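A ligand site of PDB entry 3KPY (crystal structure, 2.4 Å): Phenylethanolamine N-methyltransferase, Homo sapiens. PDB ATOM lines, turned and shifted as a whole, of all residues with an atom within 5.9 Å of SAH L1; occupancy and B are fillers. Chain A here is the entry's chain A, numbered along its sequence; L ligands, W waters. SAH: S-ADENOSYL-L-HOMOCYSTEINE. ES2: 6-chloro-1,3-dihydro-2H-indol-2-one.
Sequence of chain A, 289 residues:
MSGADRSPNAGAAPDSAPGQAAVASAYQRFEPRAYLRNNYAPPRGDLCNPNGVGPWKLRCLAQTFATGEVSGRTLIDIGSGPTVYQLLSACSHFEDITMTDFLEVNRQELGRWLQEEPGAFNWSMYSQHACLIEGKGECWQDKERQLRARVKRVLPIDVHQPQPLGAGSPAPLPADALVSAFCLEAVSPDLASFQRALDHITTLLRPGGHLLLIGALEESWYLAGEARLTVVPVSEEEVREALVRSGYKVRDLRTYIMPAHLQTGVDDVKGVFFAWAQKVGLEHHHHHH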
ATOM      1  N   ALA A  24       5.617  18.677  25.553  1.00  0.00           N
ATOM      2  CA  ALA A  24       6.033  20.055  25.289  1.00  0.00           C
ATOM      3  C   ALA A  24       6.396  20.787  26.584  1.00  0.00           C
ATOM      4  O   ALA A  24       7.125  21.791  26.558  1.00  0.00           O
ATOM      5  CB  ALA A  24       4.932  20.806  24.552  1.00  0.00           C
ATOM      6  N   TYR A  27      10.028  19.907  27.537  1.00  0.00           N
ATOM      7  CA  TYR A  27      11.075  20.785  27.012  1.00  0.00           C
ATOM      8  C   TYR A  27      11.405  21.959  27.923  1.00  0.00           C
ATOM      9  O   TYR A  27      12.346  22.705  27.646  1.00  0.00           O
ATOM     10  CB  TYR A  27      10.743  21.257  25.601  1.00  0.00           C
ATOM     11  CG  TYR A  27      11.244  20.276  24.549  1.00  0.00           C
ATOM     12  CD1 TYR A  27      10.377  19.361  23.980  1.00  0.00           C
ATOM     13  CD2 TYR A  27      12.579  20.248  24.176  1.00  0.00           C
ATOM     14  CE1 TYR A  27      10.820  18.456  23.046  1.00  0.00           C
ATOM     15  CE2 TYR A  27      13.029  19.353  23.231  1.00  0.00           C
ATOM     16  CZ  TYR A  27      12.150  18.457  22.671  1.00  0.00           C
ATOM     17  OH  TYR A  27      12.573  17.549  21.739  1.00  0.00           O
ATOM     18  N   PHE A  30      14.650  21.054  29.674  1.00  0.00           N
ATOM     19  CA  PHE A  30      15.732  20.844  28.709  1.00  0.00           C
ATOM     20  C   PHE A  30      16.958  21.697  29.040  1.00  0.00           C
ATOM     21  O   PHE A  30      16.883  22.923  29.011  1.00  0.00           O
ATOM     22  CB  PHE A  30      15.209  21.165  27.313  1.00  0.00           C
ATOM     23  CG  PHE A  30      16.207  21.019  26.217  1.00  0.00           C
ATOM     24  CD1 PHE A  30      16.114  19.973  25.309  1.00  0.00           C
ATOM     25  CD2 PHE A  30      17.226  21.951  26.052  1.00  0.00           C
ATOM     26  CE1 PHE A  30      17.016  19.840  24.281  1.00  0.00           C
ATOM     27  CE2 PHE A  30      18.148  21.821  25.022  1.00  0.00           C
ATOM     28  CZ  PHE A  30      18.038  20.765  24.137  1.00  0.00           C
ATOM     29  N   TYR A  35      22.720  18.838  26.747  1.00  0.00           N
ATOM     30  CA  TYR A  35      22.487  18.364  25.389  1.00  0.00           C
ATOM     31  C   TYR A  35      23.730  18.441  24.507  1.00  0.00           C
ATOM     32  O   TYR A  35      24.048  17.496  23.771  1.00  0.00           O
ATOM     33  CB  TYR A  35      21.323  19.125  24.748  1.00  0.00           C
ATOM     34  CG  TYR A  35      21.091  18.783  23.293  1.00  0.00           C
ATOM     35  CD1 TYR A  35      20.347  17.666  22.940  1.00  0.00           C
ATOM     36  CD2 TYR A  35      21.598  19.588  22.280  1.00  0.00           C
ATOM     37  CE1 TYR A  35      20.123  17.358  21.601  1.00  0.00           C
ATOM     38  CE2 TYR A  35      21.384  19.283  20.951  1.00  0.00           C
ATOM     39  CZ  TYR A  35      20.641  18.177  20.616  1.00  0.00           C
ATOM     40  OH  TYR A  35      20.425  17.882  19.286  1.00  0.00           O
ATOM     41  N   TYR A  40      27.563  16.486  21.343  1.00  0.00           N
ATOM     42  CA  TYR A  40      28.575  17.223  20.595  1.00  0.00           C
ATOM     43  C   TYR A  40      29.933  17.281  21.292  1.00  0.00           C
ATOM     44  O   TYR A  40      30.841  17.983  20.841  1.00  0.00           O
ATOM     45  CB  TYR A  40      28.043  18.607  20.215  1.00  0.00           C
ATOM     46  CG  TYR A  40      26.855  18.459  19.281  1.00  0.00           C
ATOM     47  CD1 TYR A  40      25.555  18.534  19.756  1.00  0.00           C
ATOM     48  CD2 TYR A  40      27.054  18.175  17.941  1.00  0.00           C
ATOM     49  CE1 TYR A  40      24.480  18.371  18.904  1.00  0.00           C
ATOM     50  CE2 TYR A  40      25.989  18.003  17.089  1.00  0.00           C
ATOM     51  CZ  TYR A  40      24.707  18.102  17.570  1.00  0.00           C
ATOM     52  OH  TYR A  40      23.642  17.929  16.708  1.00  0.00           O
ATOM     53  N   LYS A  57      27.458  13.708   9.155  1.00  0.00           N
ATOM     54  CA  LYS A  57      26.526  14.825   9.046  1.00  0.00           C
ATOM     55  C   LYS A  57      27.108  16.003   8.275  1.00  0.00           C
ATOM     56  O   LYS A  57      26.475  16.530   7.350  1.00  0.00           O
ATOM     57  CB  LYS A  57      26.056  15.266  10.432  1.00  0.00           C
ATOM     58  CG  LYS A  57      25.182  14.230  11.133  1.00  0.00           C
ATOM     59  CD  LYS A  57      24.370  14.815  12.270  1.00  0.00           C
ATOM     60  CE  LYS A  57      25.257  15.363  13.377  1.00  0.00           C
ATOM     61  NZ  LYS A  57      24.458  16.015  14.445  1.00  0.00           N
ATOM     62  N   ASP A  77      16.802  28.221   9.654  1.00  0.00           N
ATOM     63  CA  ASP A  77      17.126  26.982  10.359  1.00  0.00           C
ATOM     64  C   ASP A  77      16.048  26.712  11.391  1.00  0.00           C
ATOM     65  O   ASP A  77      15.832  27.508  12.307  1.00  0.00           O
ATOM     66  CB  ASP A  77      18.503  27.100  11.027  1.00  0.00           C
ATOM     67  CG  ASP A  77      18.967  25.803  11.645  1.00  0.00           C
ATOM     68  OD1 ASP A  77      18.596  24.725  11.131  1.00  0.00           O
ATOM     69  OD2 ASP A  77      19.700  25.847  12.644  1.00  0.00           O
ATOM     70  N   ILE A  78      15.360  25.574  11.247  1.00  0.00           N
ATOM     71  CA  ILE A  78      14.235  25.206  12.093  1.00  0.00           C
ATOM     72  C   ILE A  78      14.688  24.342  13.267  1.00  0.00           C
ATOM     73  O   ILE A  78      15.199  23.240  13.068  1.00  0.00           O
ATOM     74  CB  ILE A  78      13.176  24.391  11.297  1.00  0.00           C
ATOM     75  CG1 ILE A  78      12.822  25.082   9.972  1.00  0.00           C
ATOM     76  CG2 ILE A  78      11.932  24.148  12.149  1.00  0.00           C
ATOM     77  CD1 ILE A  78      12.254  26.486  10.130  1.00  0.00           C
ATOM     78  N   GLY A  79      14.498  24.839  14.489  1.00  0.00           N
ATOM     79  CA  GLY A  79      14.855  24.093  15.678  1.00  0.00           C
ATOM     80  C   GLY A  79      16.356  24.002  15.915  1.00  0.00           C
ATOM     81  O   GLY A  79      16.895  22.936  16.205  1.00  0.00           O
ATOM     82  N   SER A  80      17.023  25.149  15.787  1.00  0.00           N
ATOM     83  CA  SER A  80      18.468  25.242  15.925  1.00  0.00           C
ATOM     84  C   SER A  80      18.980  24.645  17.234  1.00  0.00           C
ATOM     85  O   SER A  80      20.073  24.065  17.283  1.00  0.00           O
ATOM     86  CB  SER A  80      18.910  26.715  15.840  1.00  0.00           C
ATOM     87  OG  SER A  80      18.410  27.338  14.668  1.00  0.00           O
ATOM     88  N   GLY A  81      18.193  24.780  18.302  1.00  0.00           N
ATOM     89  CA  GLY A  81      18.680  24.444  19.622  1.00  0.00           C
ATOM     90  C   GLY A  81      19.908  25.277  19.945  1.00  0.00           C
ATOM     91  O   GLY A  81      19.976  26.449  19.576  1.00  0.00           O
ATOM     92  N   PRO A  82      20.888  24.685  20.623  1.00  0.00           N
ATOM     93  CA  PRO A  82      22.100  25.436  20.968  1.00  0.00           C
ATOM     94  C   PRO A  82      23.236  25.131  19.999  1.00  0.00           C
ATOM     95  O   PRO A  82      24.385  25.217  20.399  1.00  0.00           O
ATOM     96  CB  PRO A  82      22.462  24.863  22.338  1.00  0.00           C
ATOM     97  CG  PRO A  82      21.647  23.553  22.479  1.00  0.00           C
ATOM     98  CD  PRO A  82      20.919  23.325  21.188  1.00  0.00           C
ATOM     99  N   THR A  83      22.922  24.739  18.760  1.00  0.00           N
ATOM    100  CA  THR A  83      23.985  24.287  17.857  1.00  0.00           C
ATOM    101  C   THR A  83      24.044  25.084  16.552  1.00  0.00           C
ATOM    102  O   THR A  83      23.019  25.568  16.073  1.00  0.00           O
ATOM    103  CB  THR A  83      23.893  22.767  17.562  1.00  0.00           C
ATOM    104  OG1 THR A  83      22.858  22.517  16.595  1.00  0.00           O
ATOM    105  CG2 THR A  83      23.608  21.974  18.846  1.00  0.00           C
ATOM    106  N   TYR A  85      26.603  23.939  13.945  1.00  0.00           N
ATOM    107  CA  TYR A  85      27.335  23.115  12.975  1.00  0.00           C
ATOM    108  C   TYR A  85      26.523  22.917  11.698  1.00  0.00           C
ATOM    109  O   TYR A  85      27.088  22.756  10.614  1.00  0.00           O
ATOM    110  CB  TYR A  85      27.645  21.739  13.556  1.00  0.00           C
ATOM    111  CG  TYR A  85      26.396  20.876  13.653  1.00  0.00           C
ATOM    112  CD1 TYR A  85      26.053  20.004  12.636  1.00  0.00           C
ATOM    113  CD2 TYR A  85      25.558  20.966  14.752  1.00  0.00           C
ATOM    114  CE1 TYR A  85      24.903  19.216  12.716  1.00  0.00           C
ATOM    115  CE2 TYR A  85      24.409  20.190  14.849  1.00  0.00           C
ATOM    116  CZ  TYR A  85      24.083  19.329  13.819  1.00  0.00           C
ATOM    117  OH  TYR A  85      22.952  18.566  13.914  1.00  0.00           O
ATOM    118  N   GLN A  86      25.212  22.895  11.852  1.00  0.00           N
ATOM    119  CA  GLN A  86      24.326  22.621  10.733  1.00  0.00           C
ATOM    120  C   GLN A  86      24.256  23.764   9.712  1.00  0.00           C
ATOM    121  O   GLN A  86      23.534  23.661   8.729  1.00  0.00           O
ATOM    122  CB  GLN A  86      22.918  22.253  11.220  1.00  0.00           C
ATOM    123  CG  GLN A  86      22.136  23.403  11.873  1.00  0.00           C
ATOM    124  CD  GLN A  86      22.339  23.480  13.372  1.00  0.00           C
ATOM    125  OE1 GLN A  86      23.349  22.999  13.903  1.00  0.00           O
ATOM    126  NE2 GLN A  86      21.384  24.089  14.065  1.00  0.00           N
ATOM    127  N   ASP A 101      14.577  28.712  17.629  1.00  0.00           N
ATOM    128  CA  ASP A 101      14.241  27.640  18.557  1.00  0.00           C
ATOM    129  C   ASP A 101      13.035  27.993  19.414  1.00  0.00           C
ATOM    130  O   ASP A 101      12.685  29.157  19.580  1.00  0.00           O
ATOM    131  CB  ASP A 101      15.416  27.284  19.462  1.00  0.00           C
ATOM    132  CG  ASP A 101      15.297  25.890  20.014  1.00  0.00           C
ATOM    133  OD1 ASP A 101      15.355  24.940  19.212  1.00  0.00           O
ATOM    134  OD2 ASP A 101      15.147  25.754  21.247  1.00  0.00           O
ATOM    135  N   PHE A 102      12.410  26.949  19.971  1.00  0.00           N
ATOM    136  CA  PHE A 102      11.256  27.088  20.840  1.00  0.00           C
ATOM    137  C   PHE A 102      11.658  27.610  22.217  1.00  0.00           C
ATOM    138  O   PHE A 102      10.941  28.409  22.825  1.00  0.00           O
ATOM    139  CB  PHE A 102      10.547  25.731  20.957  1.00  0.00           C
ATOM    140  CG  PHE A 102       9.345  25.733  21.856  1.00  0.00           C
ATOM    141  CD1 PHE A 102       8.128  26.243  21.422  1.00  0.00           C
ATOM    142  CD2 PHE A 102       9.417  25.197  23.127  1.00  0.00           C
ATOM    143  CE1 PHE A 102       7.020  26.243  22.252  1.00  0.00           C
ATOM    144  CE2 PHE A 102       8.311  25.186  23.959  1.00  0.00           C
ATOM    145  CZ  PHE A 102       7.112  25.709  23.521  1.00  0.00           C
ATOM    146  N   LEU A 103      12.826  27.189  22.696  1.00  0.00           N
ATOM    147  CA  LEU A 103      13.304  27.565  24.022  1.00  0.00           C
ATOM    148  C   LEU A 103      14.178  28.811  24.056  1.00  0.00           C
ATOM    149  O   LEU A 103      15.129  28.956  23.283  1.00  0.00           O
ATOM    150  CB  LEU A 103      14.077  26.410  24.676  1.00  0.00           C
ATOM    151  CG  LEU A 103      13.279  25.179  25.069  1.00  0.00           C
ATOM    152  CD1 LEU A 103      14.217  24.081  25.539  1.00  0.00           C
ATOM    153  CD2 LEU A 103      12.252  25.524  26.164  1.00  0.00           C
ATOM    154  N   ASN A 106      17.949  28.109  24.752  1.00  0.00           N
ATOM    155  CA  ASN A 106      18.688  27.769  23.542  1.00  0.00           C
ATOM    156  C   ASN A 106      19.055  29.001  22.733  1.00  0.00           C
ATOM    157  O   ASN A 106      20.152  29.092  22.196  1.00  0.00           O
ATOM    158  CB  ASN A 106      17.899  26.794  22.679  1.00  0.00           C
ATOM    159  CG  ASN A 106      18.078  25.362  23.117  1.00  0.00           C
ATOM    160  OD1 ASN A 106      17.298  24.481  22.739  1.00  0.00           O
ATOM    161  ND2 ASN A 106      19.106  25.105  23.913  1.00  0.00           N
ATOM    162  N   ILE A 157      10.039  30.110  17.890  1.00  0.00           N
ATOM    163  CA  ILE A 157       9.334  29.344  16.863  1.00  0.00           C
ATOM    164  C   ILE A 157       8.636  28.141  17.466  1.00  0.00           C
ATOM    165  O   ILE A 157       9.130  27.546  18.433  1.00  0.00           O
ATOM    166  CB  ILE A 157      10.306  28.877  15.758  1.00  0.00           C
ATOM    167  CG1 ILE A 157       9.535  28.201  14.615  1.00  0.00           C
ATOM    168  CG2 ILE A 157      11.373  27.953  16.336  1.00  0.00           C
ATOM    169  CD1 ILE A 157      10.437  27.606  13.541  1.00  0.00           C
ATOM    170  N   ASP A 158       7.497  27.786  16.906  1.00  0.00           N
ATOM    171  CA  ASP A 158       6.777  26.578  17.299  1.00  0.00           C
ATOM    172  C   ASP A 158       6.198  25.911  16.067  1.00  0.00           C
ATOM    173  O   ASP A 158       5.274  26.425  15.433  1.00  0.00           O
ATOM    174  CB  ASP A 158       5.649  26.904  18.274  1.00  0.00           C
ATOM    175  CG  ASP A 158       4.874  25.671  18.696  1.00  0.00           C
ATOM    176  OD1 ASP A 158       5.117  24.590  18.125  1.00  0.00           O
ATOM    177  OD2 ASP A 158       4.024  25.780  19.611  1.00  0.00           O
ATOM    178  N   VAL A 159       6.742  24.748  15.721  1.00  0.00           N
ATOM    179  CA  VAL A 159       6.368  24.072  14.492  1.00  0.00           C
ATOM    180  C   VAL A 159       4.942  23.505  14.560  1.00  0.00           C
ATOM    181  O   VAL A 159       4.347  23.183  13.530  1.00  0.00           O
ATOM    182  CB  VAL A 159       7.355  22.936  14.152  1.00  0.00           C
ATOM    183  CG1 VAL A 159       8.744  23.502  13.926  1.00  0.00           C
ATOM    184  CG2 VAL A 159       7.358  21.904  15.257  1.00  0.00           C
ATOM    185  N   HIS A 160       4.422  23.381  15.775  1.00  0.00           N
ATOM    186  CA  HIS A 160       3.045  22.903  15.939  1.00  0.00           C
ATOM    187  C   HIS A 160       2.046  23.967  15.520  1.00  0.00           C
ATOM    188  O   HIS A 160       0.867  23.673  15.320  1.00  0.00           O
ATOM    189  CB  HIS A 160       2.808  22.460  17.390  1.00  0.00           C
ATOM    190  CG  HIS A 160       3.685  21.327  17.809  1.00  0.00           C
ATOM    191  ND1 HIS A 160       3.908  20.220  17.020  1.00  0.00           N
ATOM    192  CD2 HIS A 160       4.398  21.119  18.951  1.00  0.00           C
ATOM    193  CE1 HIS A 160       4.724  19.383  17.642  1.00  0.00           C
ATOM    194  NE2 HIS A 160       5.032  19.910  18.815  1.00  0.00           N
ATOM    195  N   SER A 180      16.778  21.945   8.921  1.00  0.00           N
ATOM    196  CA  SER A 180      16.256  21.534  10.212  1.00  0.00           C
ATOM    197  C   SER A 180      16.853  20.213  10.618  1.00  0.00           C
ATOM    198  O   SER A 180      16.779  19.228   9.873  1.00  0.00           O
ATOM    199  CB  SER A 180      14.735  21.432  10.203  1.00  0.00           C
ATOM    200  OG  SER A 180      14.259  21.046  11.476  1.00  0.00           O
ATOM    201  N   ALA A 181      17.446  20.176  11.812  1.00  0.00           N
ATOM    202  CA  ALA A 181      18.141  18.976  12.256  1.00  0.00           C
ATOM    203  C   ALA A 181      17.652  18.549  13.636  1.00  0.00           C
ATOM    204  O   ALA A 181      17.763  19.299  14.608  1.00  0.00           O
ATOM    205  CB  ALA A 181      19.653  19.208  12.260  1.00  0.00           C
ATOM    206  N   PHE A 182      17.098  17.330  13.682  1.00  0.00           N
ATOM    207  CA  PHE A 182      16.693  16.709  14.936  1.00  0.00           C
ATOM    208  C   PHE A 182      15.617  17.486  15.671  1.00  0.00           C
ATOM    209  O   PHE A 182      15.535  17.430  16.899  1.00  0.00           O
ATOM    210  CB  PHE A 182      17.901  16.481  15.843  1.00  0.00           C
ATOM    211  CG  PHE A 182      18.977  15.644  15.217  1.00  0.00           C
ATOM    212  CD1 PHE A 182      20.112  16.247  14.666  1.00  0.00           C
ATOM    213  CD2 PHE A 182      18.861  14.267  15.160  1.00  0.00           C
ATOM    214  CE1 PHE A 182      21.103  15.474  14.091  1.00  0.00           C
ATOM    215  CE2 PHE A 182      19.853  13.493  14.585  1.00  0.00           C
ATOM    216  CZ  PHE A 182      20.978  14.097  14.045  1.00  0.00           C
ATOM    217  N   CYS A 183      14.811  18.230  14.928  1.00  0.00           N
ATOM    218  CA  CYS A 183      13.698  18.947  15.531  1.00  0.00           C
ATOM    219  C   CYS A 183      12.374  18.186  15.441  1.00  0.00           C
ATOM    220  O   CYS A 183      11.851  17.703  16.447  1.00  0.00           O
ATOM    221  CB  CYS A 183      13.535  20.330  14.895  1.00  0.00           C
ATOM    222  SG  CYS A 183      12.236  21.329  15.644  1.00  0.00           S
ATOM    223  N   ALA A 186      11.661  14.944  17.078  1.00  0.00           N
ATOM    224  CA  ALA A 186      11.966  15.170  18.490  1.00  0.00           C
ATOM    225  C   ALA A 186      10.903  15.989  19.218  1.00  0.00           C
ATOM    226  O   ALA A 186      10.965  16.138  20.438  1.00  0.00           O
ATOM    227  CB  ALA A 186      13.337  15.852  18.625  1.00  0.00           C
ATOM    228  N   VAL A 187       9.934  16.526  18.484  1.00  0.00           N
ATOM    229  CA  VAL A 187       8.890  17.347  19.099  1.00  0.00           C
ATOM    230  C   VAL A 187       7.483  16.843  18.774  1.00  0.00           C
ATOM    231  O   VAL A 187       6.490  17.461  19.135  1.00  0.00           O
ATOM    232  CB  VAL A 187       8.997  18.832  18.659  1.00  0.00           C
ATOM    233  CG1 VAL A 187      10.398  19.353  18.862  1.00  0.00           C
ATOM    234  CG2 VAL A 187       8.550  19.008  17.213  1.00  0.00           C
ATOM    235  N   TYR A 222      15.319  10.719  24.266  1.00  0.00           N
ATOM    236  CA  TYR A 222      16.676  11.168  24.522  1.00  0.00           C
ATOM    237  C   TYR A 222      16.677  12.088  25.726  1.00  0.00           C
ATOM    238  O   TYR A 222      15.648  12.671  26.085  1.00  0.00           O
ATOM    239  CB  TYR A 222      17.267  11.862  23.302  1.00  0.00           C
ATOM    240  CG  TYR A 222      16.746  13.249  23.032  1.00  0.00           C
ATOM    241  CD1 TYR A 222      17.474  14.368  23.428  1.00  0.00           C
ATOM    242  CD2 TYR A 222      15.557  13.453  22.359  1.00  0.00           C
ATOM    243  CE1 TYR A 222      17.022  15.645  23.175  1.00  0.00           C
ATOM    244  CE2 TYR A 222      15.092  14.738  22.096  1.00  0.00           C
ATOM    245  CZ  TYR A 222      15.836  15.830  22.504  1.00  0.00           C
ATOM    246  OH  TYR A 222      15.402  17.121  22.257  1.00  0.00           O
HETATM  247  N   SAH L   1      19.315  21.748  15.709  1.00  0.00           N
HETATM  248  CA  SAH L   1      19.763  20.984  16.872  1.00  0.00           C
HETATM  249  CB  SAH L   1      18.577  20.132  17.367  1.00  0.00           C
HETATM  250  CG  SAH L   1      18.123  20.654  18.731  1.00  0.00           C
HETATM  251  SD  SAH L   1      17.204  19.320  19.563  1.00  0.00           S
HETATM  252  C   SAH L   1      20.863  20.024  16.400  1.00  0.00           C
HETATM  253  O   SAH L   1      20.917  19.698  15.261  1.00  0.00           O
HETATM  254  OXT SAH L   1      21.545  19.253  17.360  1.00  0.00           O
HETATM  255  C5' SAH L   1      15.409  19.572  19.354  1.00  0.00           C
HETATM  256  C4' SAH L   1      15.094  21.080  19.354  1.00  0.00           C
HETATM  257  O4' SAH L   1      13.670  21.300  19.065  1.00  0.00           O
HETATM  258  C3' SAH L   1      15.385  21.726  20.717  1.00  0.00           C
HETATM  259  O3' SAH L   1      16.259  22.820  20.556  1.00  0.00           O
HETATM  260  C2' SAH L   1      14.017  22.172  21.143  1.00  0.00           C
HETATM  261  O2' SAH L   1      13.967  23.238  22.062  1.00  0.00           O
HETATM  262  C1' SAH L   1      13.285  22.462  19.841  1.00  0.00           C
HETATM  263  N9  SAH L   1      11.856  22.434  20.108  1.00  0.00           N
HETATM  264  C8  SAH L   1      11.199  21.818  21.294  1.00  0.00           C
HETATM  265  N7  SAH L   1       9.758  21.966  21.126  1.00  0.00           N
HETATM  266  C5  SAH L   1       9.512  22.637  19.845  1.00  0.00           C
HETATM  267  C6  SAH L   1       8.250  23.052  19.153  1.00  0.00           C
HETATM  268  N6  SAH L   1       6.958  22.757  19.773  1.00  0.00           N
HETATM  269  N1  SAH L   1       8.320  23.720  17.863  1.00  0.00           N
HETATM  270  C2  SAH L   1       9.651  24.009  17.220  1.00  0.00           C
HETATM  271  N3  SAH L   1      10.900  23.612  17.911  1.00  0.00           N
HETATM  272  C4  SAH L   1      10.826  22.925  19.224  1.00  0.00           C
HETATM  273  C10 ES2 L   2      21.602  12.882  17.814  1.00  0.00           C
HETATM  274 CL01 ES2 L   2      17.953  13.084  19.724  1.00  0.00          CL
HETATM  275  C02 ES2 L   2      19.466  13.523  18.895  1.00  0.00           C
HETATM  276  C03 ES2 L   2      19.752  14.953  18.627  1.00  0.00           C
HETATM  277  C04 ES2 L   2      20.956  15.330  17.954  1.00  0.00           C
HETATM  278  C05 ES2 L   2      21.889  14.311  17.545  1.00  0.00           C
HETATM  279  C06 ES2 L   2      23.219  14.385  16.797  1.00  0.00           C
HETATM  280  C07 ES2 L   2      23.567  12.947  16.452  1.00  0.00           C
HETATM  281  O08 ES2 L   2      24.655  12.681  16.110  1.00  0.00           O
HETATM  282  N09 ES2 L   2      22.723  12.092  17.279  1.00  0.00           N
HETATM  283  C11 ES2 L   2      20.398  12.504  18.486  1.00  0.00           C
HETATM  284  O   HOH W   1      17.047  16.123  19.090  1.00  0.00           O
HETATM  285  O   HOH W   2       7.283  21.405  22.484  1.00  0.00           O
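OH of Tyr 40 sits at hydrogen-bond distance from OH of Tyr 85, at 2.9 Å. The side-chain hydroxyl of Tyr 40 is in hydrogen-bond range of the side-chain amino group of Lys 57 (3.1 Å). N of Gly 81 is in hydrogen-bond range of OD1 of Asp 101, 3.0 Å away. N of Leu 103 lies within hydrogen-bond range of OD2 of Asp 101 (3.1 Å). N of His 160 sits at hydrogen-bond distance from OD1 of Asp 158, at 2.7 Å. O of Val 187 sits at hydrogen-bond distance from NE2 of His 160. The side-chain hydroxyl (OG1) of Thr 83 lies within hydrogen-bond range of the side-chain amide oxygen (OE1) of Gln 86 (2.8 Å). The backbone carbonyl oxygen of Ala 186 is in hydrogen-bond range of the side-chain hydroxyl of Tyr 27 (2.5 Å).
OH of Tyr 40 sits at hydrogen-bond distance from OXT of SAH L1 (2.6 Å). OXT of SAH L1 is in hydrogen-bond range of OH of Tyr 35, at 2.6 Å. The side-chain carboxylate (OD1) of Asp 101 is in hydrogen-bond range of an oxygen (O3') of SAH L1. The side-chain hydroxyl (OH) of Tyr 85 sits at hydrogen-bond distance from an oxygen (O) of SAH L1 (2.7 Å). The backbone carbonyl oxygen of Gly 79 sits at hydrogen-bond distance from a nitrogen (N) of SAH L1. The backbone NH of Val 159 is in hydrogen-bond range of a nitrogen (N1) of SAH L1 (2.9 Å). A nitrogen (N) of SAH L1 is in hydrogen-bond range of the backbone carbonyl oxygen (O) of Ser 80 (2.9 Å). The side-chain amide oxygen (OD1) of Asn 106 sits at hydrogen-bond distance from an oxygen (O3') of SAH L1 (2.9 Å). The backbone carbonyl oxygen (O) of Ala 181 sits close to a nitrogen (N) of SAH L1 (3.1 Å). N6 of SAH L1 lies within hydrogen-bond range of OD1 of Asp 158 (3.1 Å). N3 of SAH L1 sits at hydrogen-bond distance from SG of Cys 183, at 3.5 Å.
O of Phe 182 sits close to SD of SAH L1 (3.7 Å). Tyr 27 touches SAH L1 (CD2 to C8, 3.6 Å). Gly 81 touches SAH L1. Thr 83 touches SAH L1 (OG1 to C, 3.2 Å). NE2 of Gln 86 touches N of SAH L1 (3.5 Å). Phe 102 touches SAH L1 (CB to C4, 3.3 Å). Leu 103 touches SAH L1 (CD1 to O2', 3.6 Å). Ile 157 touches SAH L1 (O to C2, 3.8 Å). His 160 touches SAH L1 (CD2 to N6, 3.1 Å). Val 187 touches SAH L1 (CG1 to N7, 3.5 Å). OH of Tyr 222 touches C5' of SAH L1, 3.8 Å away. Hydrophobic or aromatic side chains that line SAH L1: Tyr 27, Tyr 35, Tyr 40, Tyr 85, Phe 102, Leu 103, Val 159, His 160, Ala 181, Phe 182 and Val 187. Within 4 Å of SAH L1: Tyr 27, Tyr 35, Tyr 40, Gly 79, Ser 80, Gly 81, Thr 83, Tyr 85, Gln 86, Asp 101, Phe 102, Leu 103, Asn 106, Ile 157, Asp 158, Val 159, His 160, Ala 181, Phe 182, Cys 183, Val 187 and Tyr 222.
Water W1 bridges the backbone carbonyl oxygen (O) of Phe 182 (3.0 Å) and a sulfur (SD) of SAH L1 (3.2 Å).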
